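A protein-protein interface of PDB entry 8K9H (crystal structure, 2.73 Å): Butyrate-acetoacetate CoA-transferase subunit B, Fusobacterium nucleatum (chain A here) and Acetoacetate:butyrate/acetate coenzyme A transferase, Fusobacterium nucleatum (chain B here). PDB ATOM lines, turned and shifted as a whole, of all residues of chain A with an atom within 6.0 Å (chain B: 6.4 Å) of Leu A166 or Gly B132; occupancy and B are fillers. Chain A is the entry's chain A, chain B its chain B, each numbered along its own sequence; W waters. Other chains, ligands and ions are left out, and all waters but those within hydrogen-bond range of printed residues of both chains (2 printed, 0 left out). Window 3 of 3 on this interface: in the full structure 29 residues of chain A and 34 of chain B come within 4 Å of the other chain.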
ATOM      1  N   ASP A 113       8.308 -19.209  16.605  1.00  0.00           N
ATOM      2  CA  ASP A 113       8.140 -19.721  15.258  1.00  0.00           C
ATOM      3  C   ASP A 113       6.884 -19.145  14.614  1.00  0.00           C
ATOM      4  O   ASP A 113       6.063 -18.486  15.262  1.00  0.00           O
ATOM      5  CB  ASP A 113       8.164 -21.257  15.249  1.00  0.00           C
ATOM      6  CG  ASP A 113       7.016 -21.878  16.006  1.00  0.00           C
ATOM      7  OD1 ASP A 113       5.986 -21.201  16.235  1.00  0.00           O
ATOM      8  OD2 ASP A 113       7.147 -23.071  16.366  1.00  0.00           O
ATOM      9  N   ASN A 117       4.309 -20.612  18.448  1.00  0.00           N
ATOM     10  CA  ASN A 117       4.889 -21.425  19.502  1.00  0.00           C
ATOM     11  C   ASN A 117       6.053 -20.702  20.140  1.00  0.00           C
ATOM     12  O   ASN A 117       6.670 -19.817  19.555  1.00  0.00           O
ATOM     13  CB  ASN A 117       5.387 -22.765  18.967  1.00  0.00           C
ATOM     14  CG  ASN A 117       4.282 -23.605  18.383  1.00  0.00           C
ATOM     15  OD1 ASN A 117       3.112 -23.483  18.776  1.00  0.00           O
ATOM     16  ND2 ASN A 117       4.641 -24.469  17.438  1.00  0.00           N
ATOM     17  N   LEU A 118       6.386 -21.126  21.342  1.00  0.00           N
ATOM     18  CA  LEU A 118       7.330 -20.385  22.153  1.00  0.00           C
ATOM     19  C   LEU A 118       8.210 -21.391  22.854  1.00  0.00           C
ATOM     20  O   LEU A 118       7.698 -22.377  23.391  1.00  0.00           O
ATOM     21  CB  LEU A 118       6.588 -19.535  23.177  1.00  0.00           C
ATOM     22  CG  LEU A 118       7.454 -18.708  24.087  1.00  0.00           C
ATOM     23  CD1 LEU A 118       8.207 -17.849  23.170  1.00  0.00           C
ATOM     24  CD2 LEU A 118       6.588 -17.873  25.000  1.00  0.00           C
ATOM     25  N   ALA A 119       9.519 -21.162  22.837  1.00  0.00           N
ATOM     26  CA  ALA A 119      10.444 -21.902  23.689  1.00  0.00           C
ATOM     27  C   ALA A 119      11.220 -20.891  24.514  1.00  0.00           C
ATOM     28  O   ALA A 119      11.876 -20.010  23.950  1.00  0.00           O
ATOM     29  CB  ALA A 119      11.378 -22.782  22.861  1.00  0.00           C
ATOM     30  N   ASN A 120      11.132 -20.993  25.847  1.00  0.00           N
ATOM     31  CA  ASN A 120      11.812 -19.966  26.642  1.00  0.00           C
ATOM     32  C   ASN A 120      12.050 -20.373  28.088  1.00  0.00           C
ATOM     33  O   ASN A 120      12.271 -19.491  28.920  1.00  0.00           O
ATOM     34  CB  ASN A 120      11.026 -18.638  26.569  1.00  0.00           C
ATOM     35  CG  ASN A 120       9.969 -18.466  27.673  1.00  0.00           C
ATOM     36  OD1 ASN A 120       9.578 -19.406  28.388  1.00  0.00           O
ATOM     37  ND2 ASN A 120       9.493 -17.235  27.800  1.00  0.00           N
ATOM     38  N   TRP A 121      11.989 -21.639  28.433  1.00  0.00           N
ATOM     39  CA  TRP A 121      12.133 -22.019  29.829  1.00  0.00           C
ATOM     40  C   TRP A 121      13.204 -23.065  30.047  1.00  0.00           C
ATOM     41  O   TRP A 121      13.600 -23.269  31.200  1.00  0.00           O
ATOM     42  CB  TRP A 121      10.798 -22.538  30.400  1.00  0.00           C
ATOM     43  CG  TRP A 121      10.366 -23.829  29.789  1.00  0.00           C
ATOM     44  CD1 TRP A 121       9.833 -24.012  28.533  1.00  0.00           C
ATOM     45  CD2 TRP A 121      10.451 -25.121  30.379  1.00  0.00           C
ATOM     46  NE1 TRP A 121       9.592 -25.351  28.309  1.00  0.00           N
ATOM     47  CE2 TRP A 121       9.956 -26.054  29.429  1.00  0.00           C
ATOM     48  CE3 TRP A 121      10.893 -25.588  31.621  1.00  0.00           C
ATOM     49  CZ2 TRP A 121       9.881 -27.426  29.691  1.00  0.00           C
ATOM     50  CZ3 TRP A 121      10.820 -26.953  31.881  1.00  0.00           C
ATOM     51  CH2 TRP A 121      10.312 -27.853  30.918  1.00  0.00           C
ATOM     52  N   MET A 135       4.310 -20.367  31.538  1.00  0.00           N
ATOM     53  CA  MET A 135       3.305 -21.138  30.805  1.00  0.00           C
ATOM     54  C   MET A 135       1.918 -20.565  31.037  1.00  0.00           C
ATOM     55  O   MET A 135       1.139 -20.389  30.090  1.00  0.00           O
ATOM     56  CB  MET A 135       3.339 -22.641  31.180  1.00  0.00           C
ATOM     57  CG  MET A 135       4.235 -23.484  30.310  1.00  0.00           C
ATOM     58  SD  MET A 135       4.729 -25.139  30.777  1.00  0.00           S
ATOM     59  CE  MET A 135       3.150 -25.735  30.959  1.00  0.00           C
ATOM     60  N   CYS A 162       9.801 -24.203  16.058  1.00  0.00           N
ATOM     61  CA  CYS A 162      10.733 -24.267  17.187  1.00  0.00           C
ATOM     62  C   CYS A 162      11.366 -25.640  17.300  1.00  0.00           C
ATOM     63  O   CYS A 162      10.790 -26.664  16.917  1.00  0.00           O
ATOM     64  CB  CYS A 162      10.046 -23.973  18.549  1.00  0.00           C
ATOM     65  SG  CYS A 162       9.379 -22.292  18.920  1.00  0.00           S
ATOM     66  N   LEU A 164      13.576 -26.168  20.319  1.00  0.00           N
ATOM     67  CA  LEU A 164      13.740 -26.304  21.750  1.00  0.00           C
ATOM     68  C   LEU A 164      12.424 -26.734  22.390  1.00  0.00           C
ATOM     69  O   LEU A 164      11.362 -26.714  21.756  1.00  0.00           O
ATOM     70  CB  LEU A 164      14.237 -24.978  22.327  1.00  0.00           C
ATOM     71  CG  LEU A 164      15.718 -24.625  22.149  1.00  0.00           C
ATOM     72  CD1 LEU A 164      15.953 -23.131  22.405  1.00  0.00           C
ATOM     73  CD2 LEU A 164      16.592 -25.484  23.058  1.00  0.00           C
ATOM     74  N   PRO A 165      12.469 -27.137  23.663  1.00  0.00           N
ATOM     75  CA  PRO A 165      11.235 -27.474  24.388  1.00  0.00           C
ATOM     76  C   PRO A 165      10.272 -26.301  24.451  1.00  0.00           C
ATOM     77  O   PRO A 165      10.643 -25.182  24.814  1.00  0.00           O
ATOM     78  CB  PRO A 165      11.746 -27.850  25.779  1.00  0.00           C
ATOM     79  CG  PRO A 165      13.119 -28.332  25.529  1.00  0.00           C
ATOM     80  CD  PRO A 165      13.662 -27.453  24.459  1.00  0.00           C
ATOM     81  N   LEU A 166       9.019 -26.576  24.121  1.00  0.00           N
ATOM     82  CA  LEU A 166       8.028 -25.518  24.079  1.00  0.00           C
ATOM     83  C   LEU A 166       7.710 -24.998  25.473  1.00  0.00           C
ATOM     84  O   LEU A 166       7.739 -25.733  26.469  1.00  0.00           O
ATOM     85  CB  LEU A 166       6.752 -26.015  23.403  1.00  0.00           C
ATOM     86  CG  LEU A 166       6.996 -26.201  21.907  1.00  0.00           C
ATOM     87  CD1 LEU A 166       5.724 -26.466  21.156  1.00  0.00           C
ATOM     88  CD2 LEU A 166       7.663 -24.965  21.368  1.00  0.00           C
ATOM     89  N   THR A 167       7.440 -23.696  25.531  1.00  0.00           N
ATOM     90  CA  THR A 167       6.715 -23.129  26.660  1.00  0.00           C
ATOM     91  C   THR A 167       5.215 -23.277  26.457  1.00  0.00           C
ATOM     92  O   THR A 167       4.506 -23.776  27.332  1.00  0.00           O
ATOM     93  CB  THR A 167       7.080 -21.660  26.843  1.00  0.00           C
ATOM     94  OG1 THR A 167       8.504 -21.534  26.927  1.00  0.00           O
ATOM     95  CG2 THR A 167       6.435 -21.113  28.107  1.00  0.00           C
ATOM     96  N   ALA A 168       4.719 -22.877  25.298  1.00  0.00           N
ATOM     97  CA  ALA A 168       3.308 -23.020  24.989  1.00  0.00           C
ATOM     98  C   ALA A 168       3.146 -23.116  23.476  1.00  0.00           C
ATOM     99  O   ALA A 168       4.085 -22.880  22.708  1.00  0.00           O
ATOM    100  CB  ALA A 168       2.500 -21.856  25.568  1.00  0.00           C
ATOM    101  N   VAL A 169       1.936 -23.437  23.050  1.00  0.00           N
ATOM    102  CA  VAL A 169       1.635 -23.642  21.640  1.00  0.00           C
ATOM    103  C   VAL A 169       0.723 -22.515  21.175  1.00  0.00           C
ATOM    104  O   VAL A 169      -0.207 -22.125  21.886  1.00  0.00           O
ATOM    105  CB  VAL A 169       1.006 -25.039  21.418  1.00  0.00           C
ATOM    106  CG1 VAL A 169       0.693 -25.272  19.983  1.00  0.00           C
ATOM    107  CG2 VAL A 169       1.951 -26.118  21.901  1.00  0.00           C
ATOM    108  N   GLY B 130       0.106 -26.091  29.812  1.00  0.00           N
ATOM    109  CA  GLY B 130       0.837 -27.341  29.684  1.00  0.00           C
ATOM    110  C   GLY B 130       0.733 -27.966  28.311  1.00  0.00           C
ATOM    111  O   GLY B 130       1.639 -28.699  27.902  1.00  0.00           O
ATOM    112  N   LEU B 131      -0.364 -27.693  27.600  1.00  0.00           N
ATOM    113  CA  LEU B 131      -0.678 -28.382  26.361  1.00  0.00           C
ATOM    114  C   LEU B 131       0.464 -28.268  25.378  1.00  0.00           C
ATOM    115  O   LEU B 131       0.931 -27.164  25.075  1.00  0.00           O
ATOM    116  CB  LEU B 131      -1.936 -27.794  25.736  1.00  0.00           C
ATOM    117  CG  LEU B 131      -3.329 -28.279  26.119  1.00  0.00           C
ATOM    118  CD1 LEU B 131      -4.361 -27.605  25.202  1.00  0.00           C
ATOM    119  CD2 LEU B 131      -3.434 -29.798  26.034  1.00  0.00           C
ATOM    120  N   GLY B 132       0.896 -29.418  24.867  1.00  0.00           N
ATOM    121  CA  GLY B 132       1.893 -29.463  23.818  1.00  0.00           C
ATOM    122  C   GLY B 132       3.293 -29.292  24.320  1.00  0.00           C
ATOM    123  O   GLY B 132       4.188 -28.962  23.535  1.00  0.00           O
ATOM    124  N   THR B 133       3.501 -29.481  25.616  1.00  0.00           N
ATOM    125  CA  THR B 133       4.780 -29.288  26.267  1.00  0.00           C
ATOM    126  C   THR B 133       5.085 -30.523  27.096  1.00  0.00           C
ATOM    127  O   THR B 133       4.322 -31.491  27.121  1.00  0.00           O
ATOM    128  CB  THR B 133       4.783 -28.049  27.169  1.00  0.00           C
ATOM    129  OG1 THR B 133       4.251 -28.399  28.457  1.00  0.00           O
ATOM    130  CG2 THR B 133       3.969 -26.911  26.545  1.00  0.00           C
ATOM    131  N   ILE B 134       6.220 -30.478  27.782  1.00  0.00           N
ATOM    132  CA  ILE B 134       6.658 -31.614  28.576  1.00  0.00           C
ATOM    133  C   ILE B 134       5.667 -31.873  29.699  1.00  0.00           C
ATOM    134  O   ILE B 134       5.522 -33.011  30.164  1.00  0.00           O
ATOM    135  CB  ILE B 134       8.092 -31.361  29.102  1.00  0.00           C
ATOM    136  CG1 ILE B 134       9.102 -31.176  27.940  1.00  0.00           C
ATOM    137  CG2 ILE B 134       8.534 -32.456  30.045  1.00  0.00           C
ATOM    138  CD1 ILE B 134       8.968 -32.176  26.781  1.00  0.00           C
ATOM    139  N   VAL B 135       4.946 -30.833  30.131  1.00  0.00           N
ATOM    140  CA  VAL B 135       4.008 -30.974  31.240  1.00  0.00           C
ATOM    141  C   VAL B 135       2.860 -31.915  30.877  1.00  0.00           C
ATOM    142  O   VAL B 135       2.363 -32.665  31.729  1.00  0.00           O
ATOM    143  CB  VAL B 135       3.507 -29.582  31.669  1.00  0.00           C
ATOM    144  CG1 VAL B 135       2.507 -29.696  32.822  1.00  0.00           C
ATOM    145  CG2 VAL B 135       4.675 -28.712  32.077  1.00  0.00           C
ATOM    146  N   GLN B 136       2.451 -31.923  29.603  1.00  0.00           N
ATOM    147  CA  GLN B 136       1.424 -32.842  29.130  1.00  0.00           C
ATOM    148  C   GLN B 136       1.771 -34.307  29.378  1.00  0.00           C
ATOM    149  O   GLN B 136       0.867 -35.125  29.563  1.00  0.00           O
ATOM    150  CB  GLN B 136       1.189 -32.632  27.644  1.00  0.00           C
ATOM    151  CG  GLN B 136       0.017 -33.402  27.102  1.00  0.00           C
ATOM    152  CD  GLN B 136      -0.400 -32.925  25.722  1.00  0.00           C
ATOM    153  OE1 GLN B 136      -0.451 -31.720  25.441  1.00  0.00           O
ATOM    154  NE2 GLN B 136      -0.723 -33.869  24.860  1.00  0.00           N
ATOM    155  N   LEU B 150      -5.600 -30.205  30.434  1.00  0.00           N
ATOM    156  CA  LEU B 150      -4.847 -31.189  31.198  1.00  0.00           C
ATOM    157  C   LEU B 150      -5.581 -31.447  32.503  1.00  0.00           C
ATOM    158  O   LEU B 150      -6.032 -30.505  33.166  1.00  0.00           O
ATOM    159  CB  LEU B 150      -3.408 -30.724  31.478  1.00  0.00           C
ATOM    160  CG  LEU B 150      -2.456 -30.374  30.330  1.00  0.00           C
ATOM    161  CD1 LEU B 150      -1.083 -30.161  30.878  1.00  0.00           C
ATOM    162  CD2 LEU B 150      -2.412 -31.433  29.258  1.00  0.00           C
HETATM  163  O   HOH W   1       0.667 -24.599  25.481  1.00  0.00           O
HETATM  164  O   HOH W   2       8.009 -28.579  26.267  1.00  0.00           O
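Of the 14 printed residues of chain A, 4 touch a printed residue of chain B.
Hydrophobic or aromatic side chains of chain A that line the printed part of chain B: Met A135, Leu A166 and Val A169.
Printed residues of chain B that touch a printed residue of chain A: Gly B130, Leu B131, Gly B132, Thr B133 and Val B135.
Hydrophobic or aromatic side chains of chain B that line the printed part of chain A: Val B135.
Met A135 touches Gly B130 (CE to CA, 3.1 Å).
Met A135 touches Thr B133.
Met A135 touches Val B135.
Leu A166 touches Gly B132.
Thr B133 touches Leu A166.
Thr A167 touches Thr B133 (O to CG2, 3.3 Å).
CG2 of Val A169 touches O of Leu B131 (3.5 Å).
Val A169 touches Gly B132 (CG2 to CA, 3.9 Å).
Leu A166 touches just these residues of chain B: Gly B132 and Thr B133.
Gly B132 touches two residues of chain A.
Of the printed residues of chain B, Val A169 touches Leu B131 (3.5 Å) and Gly B132 (3.9 Å).
Of the printed residues of chain B, Met A135 touches Gly B130, Thr B133 and Val B135.
Asn A120 touches none of the printed residues of chain B.
The nearest residue of chain A that does not touch Gly B132 is Ala A168 (5.9 Å).
The nearest printed residue of chain A that does not touch Gly B130 is Thr A167 (5.6 Å).
Water W1 lies within hydrogen-bond range of O of Leu B131 (2.6 Å) and N of Val A169 (3.0 Å).
Water W2 bridges the backbone carbonyl oxygen of Leu A166 and the backbone NH of Ile B134.
N of Thr A167 sits at hydrogen-bond distance from O of Leu A118 (2.5 Å).
OD1 of Asn A120 lies within hydrogen-bond range of OG1 of Thr A167, 2.8 Å away.
N of Gly B132 lies within hydrogen-bond range of OE1 of Gln B136.
O of Gly B130 is in hydrogen-bond range of OG1 of Thr B133 (2.7 Å).
N of Val B135 lies within hydrogen-bond range of OG1 of Thr B133 (3.0 Å).
The backbone carbonyl oxygen of Leu A166 is in hydrogen-bond range of the indole nitrogen of Trp A121.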
